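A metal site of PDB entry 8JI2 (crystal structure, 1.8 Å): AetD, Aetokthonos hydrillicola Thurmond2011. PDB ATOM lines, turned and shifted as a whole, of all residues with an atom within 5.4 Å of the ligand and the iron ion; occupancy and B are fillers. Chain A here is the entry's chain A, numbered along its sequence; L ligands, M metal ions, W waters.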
ATOM      1  N   PHE A  25     -15.368  18.881  15.692  1.00  0.00           N
ATOM      2  CA  PHE A  25     -16.615  19.621  16.063  1.00  0.00           C
ATOM      3  C   PHE A  25     -16.305  21.111  16.252  1.00  0.00           C
ATOM      4  O   PHE A  25     -17.053  21.967  15.781  1.00  0.00           O
ATOM      5  CB  PHE A  25     -17.189  18.971  17.317  1.00  0.00           C
ATOM      6  CG  PHE A  25     -18.547  19.462  17.690  1.00  0.00           C
ATOM      7  CD1 PHE A  25     -19.647  19.261  16.857  1.00  0.00           C
ATOM      8  CD2 PHE A  25     -18.761  20.116  18.891  1.00  0.00           C
ATOM      9  CE1 PHE A  25     -20.899  19.696  17.235  1.00  0.00           C
ATOM     10  CE2 PHE A  25     -20.023  20.546  19.261  1.00  0.00           C
ATOM     11  CZ  PHE A  25     -21.090  20.348  18.435  1.00  0.00           C
ATOM     12  N   ILE A  51     -32.271  27.331  20.620  1.00  0.00           N
ATOM     13  CA  ILE A  51     -31.934  26.439  21.751  1.00  0.00           C
ATOM     14  C   ILE A  51     -33.202  26.088  22.525  1.00  0.00           C
ATOM     15  O   ILE A  51     -33.120  25.097  23.280  1.00  0.00           O
ATOM     16  CB  ILE A  51     -30.862  27.085  22.644  1.00  0.00           C
ATOM     17  CG1 ILE A  51     -29.578  27.384  21.849  1.00  0.00           C
ATOM     18  CG2 ILE A  51     -30.585  26.165  23.814  1.00  0.00           C
ATOM     19  CD1 ILE A  51     -28.634  28.387  22.516  1.00  0.00           C
ATOM     20  N   PHE A  54     -34.202  22.527  22.469  1.00  0.00           N
ATOM     21  CA  PHE A  54     -33.213  21.614  23.072  1.00  0.00           C
ATOM     22  C   PHE A  54     -33.229  21.728  24.611  1.00  0.00           C
ATOM     23  O   PHE A  54     -33.280  20.696  25.299  1.00  0.00           O
ATOM     24  CB  PHE A  54     -31.795  21.941  22.581  1.00  0.00           C
ATOM     25  CG  PHE A  54     -30.751  21.197  23.352  1.00  0.00           C
ATOM     26  CD1 PHE A  54     -30.419  19.918  22.998  1.00  0.00           C
ATOM     27  CD2 PHE A  54     -30.235  21.730  24.539  1.00  0.00           C
ATOM     28  CE1 PHE A  54     -29.552  19.160  23.771  1.00  0.00           C
ATOM     29  CE2 PHE A  54     -29.346  20.984  25.268  1.00  0.00           C
ATOM     30  CZ  PHE A  54     -28.979  19.712  24.870  1.00  0.00           C
ATOM     31  N   ALA A  55     -33.212  22.936  25.154  1.00  0.00           N
ATOM     32  CA  ALA A  55     -32.777  23.150  26.559  1.00  0.00           C
ATOM     33  C   ALA A  55     -33.722  22.466  27.573  1.00  0.00           C
ATOM     34  O   ALA A  55     -33.209  21.905  28.592  1.00  0.00           O
ATOM     35  CB  ALA A  55     -32.601  24.611  26.883  1.00  0.00           C
ATOM     36  N   PHE A  58     -33.446  18.752  27.401  1.00  0.00           N
ATOM     37  CA  PHE A  58     -32.180  18.320  28.030  1.00  0.00           C
ATOM     38  C   PHE A  58     -32.404  18.229  29.537  1.00  0.00           C
ATOM     39  O   PHE A  58     -31.962  17.237  30.162  1.00  0.00           O
ATOM     40  CB  PHE A  58     -31.046  19.273  27.719  1.00  0.00           C
ATOM     41  CG  PHE A  58     -29.757  18.859  28.334  1.00  0.00           C
ATOM     42  CD1 PHE A  58     -29.005  17.817  27.832  1.00  0.00           C
ATOM     43  CD2 PHE A  58     -29.305  19.540  29.445  1.00  0.00           C
ATOM     44  CE1 PHE A  58     -27.790  17.477  28.416  1.00  0.00           C
ATOM     45  CE2 PHE A  58     -28.090  19.200  30.029  1.00  0.00           C
ATOM     46  CZ  PHE A  58     -27.371  18.137  29.543  1.00  0.00           C
ATOM     47  N   ASP A  86     -26.708  19.476  36.256  1.00  0.00           N
ATOM     48  CA  ASP A  86     -26.856  19.813  34.813  1.00  0.00           C
ATOM     49  C   ASP A  86     -28.337  20.118  34.504  1.00  0.00           C
ATOM     50  O   ASP A  86     -28.578  20.927  33.557  1.00  0.00           O
ATOM     51  CB  ASP A  86     -26.232  18.731  33.927  1.00  0.00           C
ATOM     52  CG  ASP A  86     -24.732  18.501  34.190  1.00  0.00           C
ATOM     53  OD1 ASP A  86     -24.075  19.423  34.715  1.00  0.00           O
ATOM     54  OD2 ASP A  86     -24.229  17.369  33.922  1.00  0.00           O
ATOM     55  N   HIS A  89     -29.894  24.048  34.405  1.00  0.00           N
ATOM     56  CA  HIS A  89     -29.349  25.057  33.472  1.00  0.00           C
ATOM     57  C   HIS A  89     -30.462  25.639  32.612  1.00  0.00           C
ATOM     58  O   HIS A  89     -30.280  26.770  32.072  1.00  0.00           O
ATOM     59  CB  HIS A  89     -28.175  24.485  32.665  1.00  0.00           C
ATOM     60  CG  HIS A  89     -27.004  24.118  33.511  1.00  0.00           C
ATOM     61  ND1 HIS A  89     -25.836  23.655  32.969  1.00  0.00           N
ATOM     62  CD2 HIS A  89     -26.823  24.158  34.860  1.00  0.00           C
ATOM     63  CE1 HIS A  89     -24.975  23.387  33.955  1.00  0.00           C
ATOM     64  NE2 HIS A  89     -25.579  23.666  35.125  1.00  0.00           N
ATOM     65  N   TRP A  90     -31.599  24.957  32.484  1.00  0.00           N
ATOM     66  CA  TRP A  90     -32.714  25.467  31.649  1.00  0.00           C
ATOM     67  C   TRP A  90     -33.191  26.815  32.170  1.00  0.00           C
ATOM     68  O   TRP A  90     -33.637  27.634  31.426  1.00  0.00           O
ATOM     69  CB  TRP A  90     -33.833  24.430  31.567  1.00  0.00           C
ATOM     70  CG  TRP A  90     -34.516  24.181  32.873  1.00  0.00           C
ATOM     71  CD1 TRP A  90     -34.033  23.453  33.935  1.00  0.00           C
ATOM     72  CD2 TRP A  90     -35.770  24.719  33.282  1.00  0.00           C
ATOM     73  NE1 TRP A  90     -34.945  23.466  34.947  1.00  0.00           N
ATOM     74  CE2 TRP A  90     -36.010  24.229  34.591  1.00  0.00           C
ATOM     75  CE3 TRP A  90     -36.730  25.524  32.678  1.00  0.00           C
ATOM     76  CZ2 TRP A  90     -37.188  24.508  35.280  1.00  0.00           C
ATOM     77  CZ3 TRP A  90     -37.888  25.812  33.376  1.00  0.00           C
ATOM     78  CH2 TRP A  90     -38.114  25.300  34.647  1.00  0.00           C
ATOM     79  N   LEU A 126     -32.424  15.632  19.524  1.00  0.00           N
ATOM     80  CA  LEU A 126     -31.120  15.173  20.034  1.00  0.00           C
ATOM     81  C   LEU A 126     -31.332  14.436  21.358  1.00  0.00           C
ATOM     82  O   LEU A 126     -30.875  13.302  21.500  1.00  0.00           O
ATOM     83  CB  LEU A 126     -30.210  16.373  20.218  1.00  0.00           C
ATOM     84  CG  LEU A 126     -28.834  16.103  20.841  1.00  0.00           C
ATOM     85  CD1 LEU A 126     -28.086  14.985  20.160  1.00  0.00           C
ATOM     86  CD2 LEU A 126     -28.001  17.371  20.771  1.00  0.00           C
ATOM     87  N   MET A 149     -21.623  13.847  25.236  1.00  0.00           N
ATOM     88  CA  MET A 149     -22.633  14.927  25.143  1.00  0.00           C
ATOM     89  C   MET A 149     -22.084  16.193  25.832  1.00  0.00           C
ATOM     90  O   MET A 149     -22.245  17.299  25.293  1.00  0.00           O
ATOM     91  CB  MET A 149     -23.919  14.441  25.800  1.00  0.00           C
ATOM     92  CG  MET A 149     -25.012  15.428  25.800  1.00  0.00           C
ATOM     93  SD  MET A 149     -25.417  15.778  24.062  1.00  0.00           S
ATOM     94  CE  MET A 149     -26.893  16.760  24.338  1.00  0.00           C
ATOM     95  N   GLU A 150     -21.448  16.039  26.980  1.00  0.00           N
ATOM     96  CA  GLU A 150     -20.929  17.192  27.774  1.00  0.00           C
ATOM     97  C   GLU A 150     -19.728  17.794  27.037  1.00  0.00           C
ATOM     98  O   GLU A 150     -19.589  19.030  27.080  1.00  0.00           O
ATOM     99  CB  GLU A 150     -20.601  16.770  29.203  1.00  0.00           C
ATOM    100  CG  GLU A 150     -21.825  16.397  29.999  1.00  0.00           C
ATOM    101  CD  GLU A 150     -22.750  17.577  30.301  1.00  0.00           C
ATOM    102  OE1 GLU A 150     -22.310  18.475  30.994  1.00  0.00           O
ATOM    103  OE2 GLU A 150     -23.854  17.632  29.765  1.00  0.00           O
ATOM    104  N   ALA A 152     -19.274  17.879  23.696  1.00  0.00           N
ATOM    105  CA  ALA A 152     -19.900  18.703  22.633  1.00  0.00           C
ATOM    106  C   ALA A 152     -20.503  19.984  23.235  1.00  0.00           C
ATOM    107  O   ALA A 152     -20.302  21.085  22.668  1.00  0.00           O
ATOM    108  CB  ALA A 152     -20.938  17.901  21.891  1.00  0.00           C
ATOM    109  N   GLY A 153     -21.257  19.851  24.308  1.00  0.00           N
ATOM    110  CA  GLY A 153     -21.886  20.994  24.988  1.00  0.00           C
ATOM    111  C   GLY A 153     -20.862  22.053  25.417  1.00  0.00           C
ATOM    112  O   GLY A 153     -21.070  23.269  25.186  1.00  0.00           O
ATOM    113  N   ILE A 156     -19.770  24.153  22.495  1.00  0.00           N
ATOM    114  CA  ILE A 156     -20.794  25.143  22.103  1.00  0.00           C
ATOM    115  C   ILE A 156     -20.734  26.340  23.055  1.00  0.00           C
ATOM    116  O   ILE A 156     -20.697  27.477  22.571  1.00  0.00           O
ATOM    117  CB  ILE A 156     -22.166  24.465  22.088  1.00  0.00           C
ATOM    118  CG1 ILE A 156     -22.206  23.421  20.964  1.00  0.00           C
ATOM    119  CG2 ILE A 156     -23.256  25.503  21.997  1.00  0.00           C
ATOM    120  CD1 ILE A 156     -23.441  22.519  21.046  1.00  0.00           C
ATOM    121  N   PHE A 157     -20.708  26.080  24.336  1.00  0.00           N
ATOM    122  CA  PHE A 157     -20.850  27.173  25.338  1.00  0.00           C
ATOM    123  C   PHE A 157     -19.542  27.930  25.514  1.00  0.00           C
ATOM    124  O   PHE A 157     -19.615  29.124  25.800  1.00  0.00           O
ATOM    125  CB  PHE A 157     -21.532  26.646  26.604  1.00  0.00           C
ATOM    126  CG  PHE A 157     -23.000  26.480  26.374  1.00  0.00           C
ATOM    127  CD1 PHE A 157     -23.879  27.556  26.469  1.00  0.00           C
ATOM    128  CD2 PHE A 157     -23.511  25.240  26.005  1.00  0.00           C
ATOM    129  CE1 PHE A 157     -25.228  27.395  26.181  1.00  0.00           C
ATOM    130  CE2 PHE A 157     -24.863  25.088  25.715  1.00  0.00           C
ATOM    131  CZ  PHE A 157     -25.716  26.151  25.801  1.00  0.00           C
ATOM    132  N   TYR A 177     -26.347  31.766  31.042  1.00  0.00           N
ATOM    133  CA  TYR A 177     -26.377  30.587  30.126  1.00  0.00           C
ATOM    134  C   TYR A 177     -25.296  30.739  29.064  1.00  0.00           C
ATOM    135  O   TYR A 177     -24.480  29.851  28.936  1.00  0.00           O
ATOM    136  CB  TYR A 177     -27.782  30.449  29.531  1.00  0.00           C
ATOM    137  CG  TYR A 177     -28.026  29.154  28.802  1.00  0.00           C
ATOM    138  CD1 TYR A 177     -28.116  27.963  29.481  1.00  0.00           C
ATOM    139  CD2 TYR A 177     -28.221  29.114  27.423  1.00  0.00           C
ATOM    140  CE1 TYR A 177     -28.388  26.750  28.850  1.00  0.00           C
ATOM    141  CE2 TYR A 177     -28.515  27.921  26.768  1.00  0.00           C
ATOM    142  CZ  TYR A 177     -28.594  26.739  27.476  1.00  0.00           C
ATOM    143  OH  TYR A 177     -28.882  25.544  26.862  1.00  0.00           O
ATOM    144  N   HIS A 182     -21.400  29.373  33.243  1.00  0.00           N
ATOM    145  CA  HIS A 182     -21.978  28.094  32.732  1.00  0.00           C
ATOM    146  C   HIS A 182     -20.850  27.121  32.350  1.00  0.00           C
ATOM    147  O   HIS A 182     -20.911  25.939  32.762  1.00  0.00           O
ATOM    148  CB  HIS A 182     -22.918  28.395  31.550  1.00  0.00           C
ATOM    149  CG  HIS A 182     -23.696  27.209  31.082  1.00  0.00           C
ATOM    150  ND1 HIS A 182     -24.506  27.323  29.970  1.00  0.00           N
ATOM    151  CD2 HIS A 182     -23.785  25.931  31.503  1.00  0.00           C
ATOM    152  CE1 HIS A 182     -25.071  26.162  29.741  1.00  0.00           C
ATOM    153  NE2 HIS A 182     -24.660  25.261  30.656  1.00  0.00           N
ATOM    154  N   GLU A 186     -20.102  23.676  34.589  1.00  0.00           N
ATOM    155  CA  GLU A 186     -20.340  22.471  33.740  1.00  0.00           C
ATOM    156  C   GLU A 186     -19.103  21.563  33.748  1.00  0.00           C
ATOM    157  O   GLU A 186     -19.267  20.363  33.965  1.00  0.00           O
ATOM    158  CB  GLU A 186     -20.692  22.838  32.302  1.00  0.00           C
ATOM    159  CG  GLU A 186     -21.338  21.714  31.520  1.00  0.00           C
ATOM    160  CD  GLU A 186     -22.854  21.748  31.417  1.00  0.00           C
ATOM    161  OE1 GLU A 186     -23.386  22.821  31.535  1.00  0.00           O
ATOM    162  OE2 GLU A 186     -23.495  20.692  31.152  1.00  0.00           O
ATOM    163  N   SER A 224     -25.029  15.944  17.406  1.00  0.00           N
ATOM    164  CA  SER A 224     -24.605  17.304  17.788  1.00  0.00           C
ATOM    165  C   SER A 224     -24.239  18.115  16.545  1.00  0.00           C
ATOM    166  O   SER A 224     -24.604  19.302  16.439  1.00  0.00           O
ATOM    167  CB  SER A 224     -23.444  17.252  18.717  1.00  0.00           C
ATOM    168  OG  SER A 224     -23.830  16.636  19.935  1.00  0.00           O
ATOM    169  N   LEU A 227     -27.437  19.187  14.842  1.00  0.00           N
ATOM    170  CA  LEU A 227     -28.018  20.336  15.580  1.00  0.00           C
ATOM    171  C   LEU A 227     -27.291  21.617  15.125  1.00  0.00           C
ATOM    172  O   LEU A 227     -27.943  22.627  14.762  1.00  0.00           O
ATOM    173  CB  LEU A 227     -27.926  20.034  17.100  1.00  0.00           C
ATOM    174  CG  LEU A 227     -28.336  21.166  18.047  1.00  0.00           C
ATOM    175  CD1 LEU A 227     -28.661  20.580  19.429  1.00  0.00           C
ATOM    176  CD2 LEU A 227     -27.240  22.225  18.187  1.00  0.00           C
ATOM    177  N   PHE A 231     -28.500  25.318  13.401  1.00  0.00           N
ATOM    178  CA  PHE A 231     -28.211  26.679  13.902  1.00  0.00           C
ATOM    179  C   PHE A 231     -27.618  27.483  12.740  1.00  0.00           C
ATOM    180  O   PHE A 231     -28.003  28.637  12.550  1.00  0.00           O
ATOM    181  CB  PHE A 231     -27.311  26.671  15.111  1.00  0.00           C
ATOM    182  CG  PHE A 231     -27.929  26.148  16.384  1.00  0.00           C
ATOM    183  CD1 PHE A 231     -29.176  25.579  16.403  1.00  0.00           C
ATOM    184  CD2 PHE A 231     -27.226  26.234  17.575  1.00  0.00           C
ATOM    185  CE1 PHE A 231     -29.717  25.046  17.572  1.00  0.00           C
ATOM    186  CE2 PHE A 231     -27.761  25.715  18.751  1.00  0.00           C
ATOM    187  CZ  PHE A 231     -29.012  25.153  18.759  1.00  0.00           C
HETATM  188  O1  LIG L   1     -28.421  23.340  28.299  1.00  0.00           O
HETATM  189  C1  LIG L   1     -27.298  23.263  28.919  1.00  0.00           C
HETATM  190  O2  LIG L   1     -27.185  23.644  30.125  1.00  0.00           O
HETATM  191  C2  LIG L   1     -26.094  22.673  28.124  1.00  0.00           C
HETATM  192  N1  LIG L   1     -24.823  22.766  28.887  1.00  0.00           N
HETATM  193  C3  LIG L   1     -26.309  21.242  27.745  1.00  0.00           C
HETATM  194  C4  LIG L   1     -25.687  20.611  26.447  1.00  0.00           C
HETATM  195  C5  LIG L   1     -25.915  21.044  25.174  1.00  0.00           C
HETATM  196  C6  LIG L   1     -26.589  22.052  24.537  1.00  0.00           C
HETATM  197  C7  LIG L   1     -26.718  22.191  23.100  1.00  0.00           C
HETATM  198 BR1  LIG L   1     -27.585  23.613  22.394  1.00  0.00          BR
HETATM  199  C8  LIG L   1     -26.078  21.211  22.388  1.00  0.00           C
HETATM  200  C9  LIG L   1     -25.447  20.247  23.070  1.00  0.00           C
HETATM  201 BR2  LIG L   1     -24.586  18.793  21.947  1.00  0.00          BR
HETATM  202  C10 LIG L   1     -25.316  20.120  24.382  1.00  0.00           C
HETATM  203  N2  LIG L   1     -24.774  19.188  25.133  1.00  0.00           N
HETATM  204  C11 LIG L   1     -24.961  19.477  26.423  1.00  0.00           C
HETATM  205 FE    FE M   1     -25.354  23.329  30.917  1.00  0.00          FE
HETATM  206  O   HOH W   1     -25.933  21.434  31.257  1.00  0.00           O
HETATM  207  O   HOH W   2     -30.816  23.002  29.810  1.00  0.00           O
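A nitrogen (N2) of the ligand sits close to the side-chain sulfur (SD) of Met 149 (3.6 Å). The side-chain hydroxyl (OH) of Tyr 177 lies within hydrogen-bond range of an oxygen (O1) of the ligand, at 2.7 Å. O of Met 149 sits at hydrogen-bond distance from N2 of the ligand, at 3.2 Å.
OE2 of Glu 186 lies close to OE1 of Glu 150. ND1 of His 182 is in hydrogen-bond range of O of Tyr 177 (2.7 Å).
CE2 of Phe 54 touches C6 of the ligand, 3.0 Å away. CE2 of Phe 58 touches C3 of the ligand, at 3.5 Å. Leu 126 touches the ligand (CD2 to BR2, 3.9 Å). Glu 150 touches the ligand (OE2 to C11, 3.97 Å). Ala 152 touches the ligand (CB to BR2, 3.8 Å). CA of Gly 153 touches N2 of the ligand, 3.4 Å away. Ile 156 touches the ligand (CD1 to C8, 3.2 Å). Phe 157 touches the ligand (CE2 to C2, 3.6 Å). Ser 224 touches the ligand (OG to BR2, 3.0 Å). Leu 227 touches the ligand. The nearest printed residue that does not touch the ligand is Ile 51 (4.2 Å).
Three residues have an atom within 4 Å of the iron ion: His 89, His 182 and Glu 186. The nearest printed residue that does not touch the iron ion is Asp 86 (4.8 Å).
The iron ion is bound by water W1 (2.0 Å), O2 of the ligand (2.0 Å), NE2 of His 182 (2.1 Å), OE1 of Glu 186 (2.1 Å), ND1 of His 89 (2.1 Å) and N1 of the ligand (2.2 Å). The iron ion has six donor atoms within binding distance.
Water W2 lies within hydrogen-bond range of an oxygen (O1) of the ligand (2.9 Å), the backbone carbonyl oxygen of Ala 55 (2.9 Å) and the backbone NH of Trp 90 (3.4 Å).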
